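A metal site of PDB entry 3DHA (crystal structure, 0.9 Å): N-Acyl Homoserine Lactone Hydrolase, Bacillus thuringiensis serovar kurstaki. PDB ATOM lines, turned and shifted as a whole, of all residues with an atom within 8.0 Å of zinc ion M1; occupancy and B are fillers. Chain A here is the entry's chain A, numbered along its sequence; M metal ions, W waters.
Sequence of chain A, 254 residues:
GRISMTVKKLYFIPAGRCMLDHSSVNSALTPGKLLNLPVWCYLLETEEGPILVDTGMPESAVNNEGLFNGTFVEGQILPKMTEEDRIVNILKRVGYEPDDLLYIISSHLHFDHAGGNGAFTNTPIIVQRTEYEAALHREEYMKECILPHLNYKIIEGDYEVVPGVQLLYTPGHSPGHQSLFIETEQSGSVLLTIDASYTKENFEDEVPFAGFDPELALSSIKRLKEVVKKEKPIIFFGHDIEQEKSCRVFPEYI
N of His 239 is in hydrogen-bond range of O of Tyr 198, 2.8 Å away.
A ring nitrogen (NE2) of His 177 is in hydrogen-bond range of the backbone NH (N) of Asp 195, at 2.9 Å.
A ring nitrogen (ND1) of His 113 sits at hydrogen-bond distance from the side-chain carboxylate (OD2) of Asp 54 (2.8 Å).
ND1 of His 113 sits at hydrogen-bond distance from OG of Ser 107 (3.4 Å).
A ring nitrogen (ND1) of His 239 is in hydrogen-bond range of the backbone carbonyl oxygen (O) of Pro 38, 2.8 Å away.
Zinc ion M1 is bound by NE2 of His 239, NE2 of His 113, water W1, OD2 of Asp 195 and OD1 of Asp 112.
Within 4 Å of zinc ion M1: Asp 112, His 113, Asp 195 and His 239.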
ATOM      1  N   CYS A  18     -30.456   4.940   4.870  1.00  0.00           N
ATOM      2  CA  CYS A  18     -29.227   5.484   4.294  1.00  0.00           C
ATOM      3  C   CYS A  18     -28.174   4.409   4.324  1.00  0.00           C
ATOM      4  O   CYS A  18     -27.927   3.781   5.363  1.00  0.00           O
ATOM      5  CB  CYS A  18     -28.805   6.716   5.079  1.00  0.00           C
ATOM      6  SG  CYS A  18     -27.442   7.632   4.315  1.00  0.00           S
ATOM      7  N   LEU A  20     -24.241   3.509   4.314  1.00  0.00           N
ATOM      8  CA  LEU A  20     -22.951   3.937   4.758  1.00  0.00           C
ATOM      9  C   LEU A  20     -22.042   2.692   4.718  1.00  0.00           C
ATOM     10  O   LEU A  20     -22.511   1.572   4.949  1.00  0.00           O
ATOM     11  CB  LEU A  20     -22.968   4.514   6.165  1.00  0.00           C
ATOM     12  CG  LEU A  20     -23.059   6.009   6.385  1.00  0.00           C
ATOM     13  CD1 LEU A  20     -23.963   6.741   5.430  1.00  0.00           C
ATOM     14  CD2 LEU A  20     -23.494   6.278   7.842  1.00  0.00           C
ATOM     15  N   LEU A  37     -28.836   1.438   6.773  1.00  0.00           N
ATOM     16  CA  LEU A  37     -29.098   1.897   8.149  1.00  0.00           C
ATOM     17  C   LEU A  37     -30.400   2.636   8.242  1.00  0.00           C
ATOM     18  O   LEU A  37     -30.786   3.336   7.300  1.00  0.00           O
ATOM     19  CB  LEU A  37     -27.935   2.806   8.582  1.00  0.00           C
ATOM     20  CG  LEU A  37     -26.560   2.232   8.575  1.00  0.00           C
ATOM     21  CD1 LEU A  37     -25.532   3.277   8.984  1.00  0.00           C
ATOM     22  CD2 LEU A  37     -26.521   1.094   9.574  1.00  0.00           C
ATOM     23  N   PRO A  38     -31.083   2.548   9.372  1.00  0.00           N
ATOM     24  CA  PRO A  38     -32.325   3.303   9.528  1.00  0.00           C
ATOM     25  C   PRO A  38     -32.067   4.779   9.719  1.00  0.00           C
ATOM     26  O   PRO A  38     -31.113   5.169  10.381  1.00  0.00           O
ATOM     27  CB  PRO A  38     -32.903   2.723  10.827  1.00  0.00           C
ATOM     28  CG  PRO A  38     -31.719   2.258  11.625  1.00  0.00           C
ATOM     29  CD  PRO A  38     -30.729   1.772  10.576  1.00  0.00           C
ATOM     30  N   VAL A  39     -32.988   5.608   9.211  1.00  0.00           N
ATOM     31  CA  VAL A  39     -33.104   7.009   9.517  1.00  0.00           C
ATOM     32  C   VAL A  39     -34.398   7.189  10.335  1.00  0.00           C
ATOM     33  O   VAL A  39     -35.433   6.674   9.954  1.00  0.00           O
ATOM     34  CB  VAL A  39     -33.087   7.861   8.253  1.00  0.00           C
ATOM     35  CG1 VAL A  39     -33.346   9.336   8.550  1.00  0.00           C
ATOM     36  CG2 VAL A  39     -31.754   7.713   7.515  1.00  0.00           C
ATOM     37  N   TRP A  40     -34.278   7.914  11.439  1.00  0.00           N
ATOM     38  CA  TRP A  40     -35.357   8.101  12.388  1.00  0.00           C
ATOM     39  C   TRP A  40     -35.795   9.535  12.541  1.00  0.00           C
ATOM     40  O   TRP A  40     -34.972  10.438  12.550  1.00  0.00           O
ATOM     41  CB  TRP A  40     -34.944   7.669  13.768  1.00  0.00           C
ATOM     42  CG  TRP A  40     -34.571   6.226  13.941  1.00  0.00           C
ATOM     43  CD1 TRP A  40     -33.351   5.710  14.081  1.00  0.00           C
ATOM     44  CD2 TRP A  40     -35.497   5.129  14.008  1.00  0.00           C
ATOM     45  NE1 TRP A  40     -33.409   4.360  14.207  1.00  0.00           N
ATOM     46  CE2 TRP A  40     -34.730   3.953  14.195  1.00  0.00           C
ATOM     47  CE3 TRP A  40     -36.886   5.011  13.933  1.00  0.00           C
ATOM     48  CZ2 TRP A  40     -35.311   2.683  14.311  1.00  0.00           C
ATOM     49  CZ3 TRP A  40     -37.479   3.759  14.054  1.00  0.00           C
ATOM     50  CH2 TRP A  40     -36.675   2.599  14.247  1.00  0.00           C
ATOM     51  N   ASP A  54     -35.917  15.769  14.763  1.00  0.00           N
ATOM     52  CA  ASP A  54     -35.298  15.526  13.449  1.00  0.00           C
ATOM     53  C   ASP A  54     -36.389  15.439  12.364  1.00  0.00           C
ATOM     54  O   ASP A  54     -37.591  15.290  12.602  1.00  0.00           O
ATOM     55  CB  ASP A  54     -34.299  14.397  13.522  1.00  0.00           C
ATOM     56  CG  ASP A  54     -33.048  14.798  14.325  1.00  0.00           C
ATOM     57  OD1 ASP A  54     -32.816  15.977  14.573  1.00  0.00           O
ATOM     58  OD2 ASP A  54     -32.283  13.820  14.671  1.00  0.00           O
ATOM     59  N   SER A 107     -31.205  17.393  16.381  1.00  0.00           N
ATOM     60  CA  SER A 107     -30.081  16.812  17.086  1.00  0.00           C
ATOM     61  C   SER A 107     -28.777  17.368  16.587  1.00  0.00           C
ATOM     62  O   SER A 107     -27.837  17.616  17.310  1.00  0.00           O
ATOM     63  CB  SER A 107     -30.091  15.289  16.970  1.00  0.00           C
ATOM     64  OG  SER A 107     -29.965  14.896  15.615  1.00  0.00           O
ATOM     65  N   HIS A 108     -28.710  17.516  15.237  1.00  0.00           N
ATOM     66  CA  HIS A 108     -27.596  18.079  14.523  1.00  0.00           C
ATOM     67  C   HIS A 108     -28.074  18.316  13.095  1.00  0.00           C
ATOM     68  O   HIS A 108     -29.188  17.982  12.764  1.00  0.00           O
ATOM     69  CB  HIS A 108     -26.354  17.190  14.647  1.00  0.00           C
ATOM     70  CG  HIS A 108     -26.426  15.808  14.081  1.00  0.00           C
ATOM     71  ND1 HIS A 108     -27.354  14.847  14.438  1.00  0.00           N
ATOM     72  CD2 HIS A 108     -25.559  15.184  13.254  1.00  0.00           C
ATOM     73  CE1 HIS A 108     -27.021  13.694  13.849  1.00  0.00           C
ATOM     74  NE2 HIS A 108     -25.942  13.850  13.089  1.00  0.00           N
ATOM     75  N   HIS A 110     -26.623  17.293  10.120  1.00  0.00           N
ATOM     76  CA  HIS A 110     -26.349  16.351   9.036  1.00  0.00           C
ATOM     77  C   HIS A 110     -27.603  16.173   8.188  1.00  0.00           C
ATOM     78  O   HIS A 110     -28.753  16.307   8.682  1.00  0.00           O
ATOM     79  CB  HIS A 110     -25.858  15.041   9.623  1.00  0.00           C
ATOM     80  CG  HIS A 110     -24.429  15.104  10.113  1.00  0.00           C
ATOM     81  ND1 HIS A 110     -23.897  14.085  10.853  1.00  0.00           N
ATOM     82  CD2 HIS A 110     -23.505  16.077   9.952  1.00  0.00           C
ATOM     83  CE1 HIS A 110     -22.633  14.432  11.135  1.00  0.00           C
ATOM     84  NE2 HIS A 110     -22.364  15.628  10.616  1.00  0.00           N
ATOM     85  N   PHE A 111     -27.383  15.734   6.958  1.00  0.00           N
ATOM     86  CA  PHE A 111     -28.477  15.696   5.981  1.00  0.00           C
ATOM     87  C   PHE A 111     -29.614  14.727   6.323  1.00  0.00           C
ATOM     88  O   PHE A 111     -30.749  14.918   5.864  1.00  0.00           O
ATOM     89  CB  PHE A 111     -27.924  15.417   4.553  1.00  0.00           C
ATOM     90  CG  PHE A 111     -27.903  13.961   4.187  1.00  0.00           C
ATOM     91  CD1 PHE A 111     -28.767  13.525   3.222  1.00  0.00           C
ATOM     92  CD2 PHE A 111     -27.070  13.015   4.786  1.00  0.00           C
ATOM     93  CE1 PHE A 111     -28.858  12.182   2.835  1.00  0.00           C
ATOM     94  CE2 PHE A 111     -27.186  11.630   4.463  1.00  0.00           C
ATOM     95  CZ  PHE A 111     -28.097  11.255   3.504  1.00  0.00           C
ATOM     96  N   ASP A 112     -29.290  13.687   7.101  1.00  0.00           N
ATOM     97  CA  ASP A 112     -30.267  12.681   7.499  1.00  0.00           C
ATOM     98  C   ASP A 112     -31.046  13.081   8.724  1.00  0.00           C
ATOM     99  O   ASP A 112     -31.909  12.315   9.127  1.00  0.00           O
ATOM    100  CB  ASP A 112     -29.553  11.313   7.633  1.00  0.00           C
ATOM    101  CG  ASP A 112     -28.359  11.292   8.582  1.00  0.00           C
ATOM    102  OD1 ASP A 112     -28.277  10.315   9.369  1.00  0.00           O
ATOM    103  OD2 ASP A 112     -27.468  12.161   8.500  1.00  0.00           O
ATOM    104  N   HIS A 113     -30.779  14.264   9.280  1.00  0.00           N
ATOM    105  CA  HIS A 113     -31.437  14.755  10.478  1.00  0.00           C
ATOM    106  C   HIS A 113     -32.109  16.082  10.263  1.00  0.00           C
ATOM    107  O   HIS A 113     -33.077  16.381  10.995  1.00  0.00           O
ATOM    108  CB  HIS A 113     -30.427  14.912  11.627  1.00  0.00           C
ATOM    109  CG  HIS A 113     -29.851  13.594  11.965  1.00  0.00           C
ATOM    110  ND1 HIS A 113     -30.347  12.797  12.955  1.00  0.00           N
ATOM    111  CD2 HIS A 113     -28.901  12.849  11.419  1.00  0.00           C
ATOM    112  CE1 HIS A 113     -29.649  11.613  12.944  1.00  0.00           C
ATOM    113  NE2 HIS A 113     -28.736  11.619  11.994  1.00  0.00           N
ATOM    114  N   HIS A 173     -19.559  13.723  17.329  1.00  0.00           N
ATOM    115  CA  HIS A 173     -19.963  13.238  16.001  1.00  0.00           C
ATOM    116  C   HIS A 173     -20.146  14.408  15.058  1.00  0.00           C
ATOM    117  O   HIS A 173     -19.830  14.297  13.871  1.00  0.00           O
ATOM    118  CB  HIS A 173     -21.245  12.454  16.150  1.00  0.00           C
ATOM    119  CG  HIS A 173     -21.899  12.139  14.832  1.00  0.00           C
ATOM    120  ND1 HIS A 173     -21.441  11.206  13.922  1.00  0.00           N
ATOM    121  CD2 HIS A 173     -23.009  12.666  14.283  1.00  0.00           C
ATOM    122  CE1 HIS A 173     -22.264  11.191  12.871  1.00  0.00           C
ATOM    123  NE2 HIS A 173     -23.281  12.038  13.045  1.00  0.00           N
ATOM    124  N   HIS A 177     -23.608  18.425  18.312  1.00  0.00           N
ATOM    125  CA  HIS A 177     -24.565  17.337  18.445  1.00  0.00           C
ATOM    126  C   HIS A 177     -25.193  17.380  19.830  1.00  0.00           C
ATOM    127  O   HIS A 177     -24.517  17.617  20.851  1.00  0.00           O
ATOM    128  CB  HIS A 177     -23.830  15.994  18.173  1.00  0.00           C
ATOM    129  CG  HIS A 177     -24.783  14.854  18.241  1.00  0.00           C
ATOM    130  ND1 HIS A 177     -25.159  14.241  19.407  1.00  0.00           N
ATOM    131  CD2 HIS A 177     -25.478  14.247  17.222  1.00  0.00           C
ATOM    132  CE1 HIS A 177     -26.059  13.314  19.107  1.00  0.00           C
ATOM    133  NE2 HIS A 177     -26.270  13.258  17.783  1.00  0.00           N
ATOM    134  N   ILE A 194     -29.182   9.538  19.773  1.00  0.00           N
ATOM    135  CA  ILE A 194     -28.996  10.011  18.404  1.00  0.00           C
ATOM    136  C   ILE A 194     -27.603   9.566  17.980  1.00  0.00           C
ATOM    137  O   ILE A 194     -27.233   8.405  18.269  1.00  0.00           O
ATOM    138  CB  ILE A 194     -29.375  11.496  18.147  1.00  0.00           C
ATOM    139  CG1 ILE A 194     -30.539  11.954  19.018  1.00  0.00           C
ATOM    140  CG2 ILE A 194     -29.601  11.722  16.653  1.00  0.00           C
ATOM    141  CD1 ILE A 194     -31.885  11.375  18.641  1.00  0.00           C
ATOM    142  N   ASP A 195     -26.823  10.405  17.340  1.00  0.00           N
ATOM    143  CA  ASP A 195     -25.582   9.963  16.772  1.00  0.00           C
ATOM    144  C   ASP A 195     -24.387  10.173  17.674  1.00  0.00           C
ATOM    145  O   ASP A 195     -23.241  10.090  17.246  1.00  0.00           O
ATOM    146  CB  ASP A 195     -25.352  10.652  15.393  1.00  0.00           C
ATOM    147  CG  ASP A 195     -26.331  10.130  14.334  1.00  0.00           C
ATOM    148  OD1 ASP A 195     -27.232   9.308  14.603  1.00  0.00           O
ATOM    149  OD2 ASP A 195     -26.162  10.616  13.187  1.00  0.00           O
ATOM    150  N   ALA A 196     -24.634  10.364  18.973  1.00  0.00           N
ATOM    151  CA  ALA A 196     -23.588  10.280  19.959  1.00  0.00           C
ATOM    152  C   ALA A 196     -23.121   8.825  20.042  1.00  0.00           C
ATOM    153  O   ALA A 196     -22.102   8.558  20.612  1.00  0.00           O
ATOM    154  CB  ALA A 196     -24.001  10.888  21.285  1.00  0.00           C
ATOM    155  N   TYR A 198     -23.789   5.560  17.070  1.00  0.00           N
ATOM    156  CA  TYR A 198     -24.599   4.931  16.043  1.00  0.00           C
ATOM    157  C   TYR A 198     -25.166   3.605  16.509  1.00  0.00           C
ATOM    158  O   TYR A 198     -26.318   3.288  16.214  1.00  0.00           O
ATOM    159  CB  TYR A 198     -23.761   4.622  14.793  1.00  0.00           C
ATOM    160  CG  TYR A 198     -23.468   5.758  13.857  1.00  0.00           C
ATOM    161  CD1 TYR A 198     -23.939   7.030  13.929  1.00  0.00           C
ATOM    162  CD2 TYR A 198     -22.658   5.491  12.789  1.00  0.00           C
ATOM    163  CE1 TYR A 198     -23.631   8.045  12.999  1.00  0.00           C
ATOM    164  CE2 TYR A 198     -22.365   6.444  11.856  1.00  0.00           C
ATOM    165  CZ  TYR A 198     -22.820   7.706  11.921  1.00  0.00           C
ATOM    166  OH  TYR A 198     -22.484   8.607  10.960  1.00  0.00           O
ATOM    167  N   GLY A 238     -28.514   5.631  17.477  1.00  0.00           N
ATOM    168  CA  GLY A 238     -28.901   6.393  16.340  1.00  0.00           C
ATOM    169  C   GLY A 238     -29.072   5.653  14.999  1.00  0.00           C
ATOM    170  O   GLY A 238     -29.979   6.024  14.233  1.00  0.00           O
ATOM    171  N   HIS A 239     -28.230   4.698  14.702  1.00  0.00           N
ATOM    172  CA  HIS A 239     -28.268   4.020  13.382  1.00  0.00           C
ATOM    173  C   HIS A 239     -27.853   2.588  13.549  1.00  0.00           C
ATOM    174  O   HIS A 239     -26.756   2.185  13.123  1.00  0.00           O
ATOM    175  CB  HIS A 239     -27.369   4.764  12.396  1.00  0.00           C
ATOM    176  CG  HIS A 239     -27.710   6.148  11.985  1.00  0.00           C
ATOM    177  ND1 HIS A 239     -28.832   6.486  11.229  1.00  0.00           N
ATOM    178  CD2 HIS A 239     -27.038   7.306  12.156  1.00  0.00           C
ATOM    179  CE1 HIS A 239     -28.781   7.784  11.009  1.00  0.00           C
ATOM    180  NE2 HIS A 239     -27.697   8.355  11.553  1.00  0.00           N
HETATM  181 ZN    ZN M   1     -27.293  10.308  11.486  1.00  0.00          ZN
HETATM  182 ZN    ZN M   2     -24.869  12.550  11.954  1.00  0.00          ZN
HETATM  183  O   HOH W   1     -25.797  11.400  10.690  1.00  0.00           O
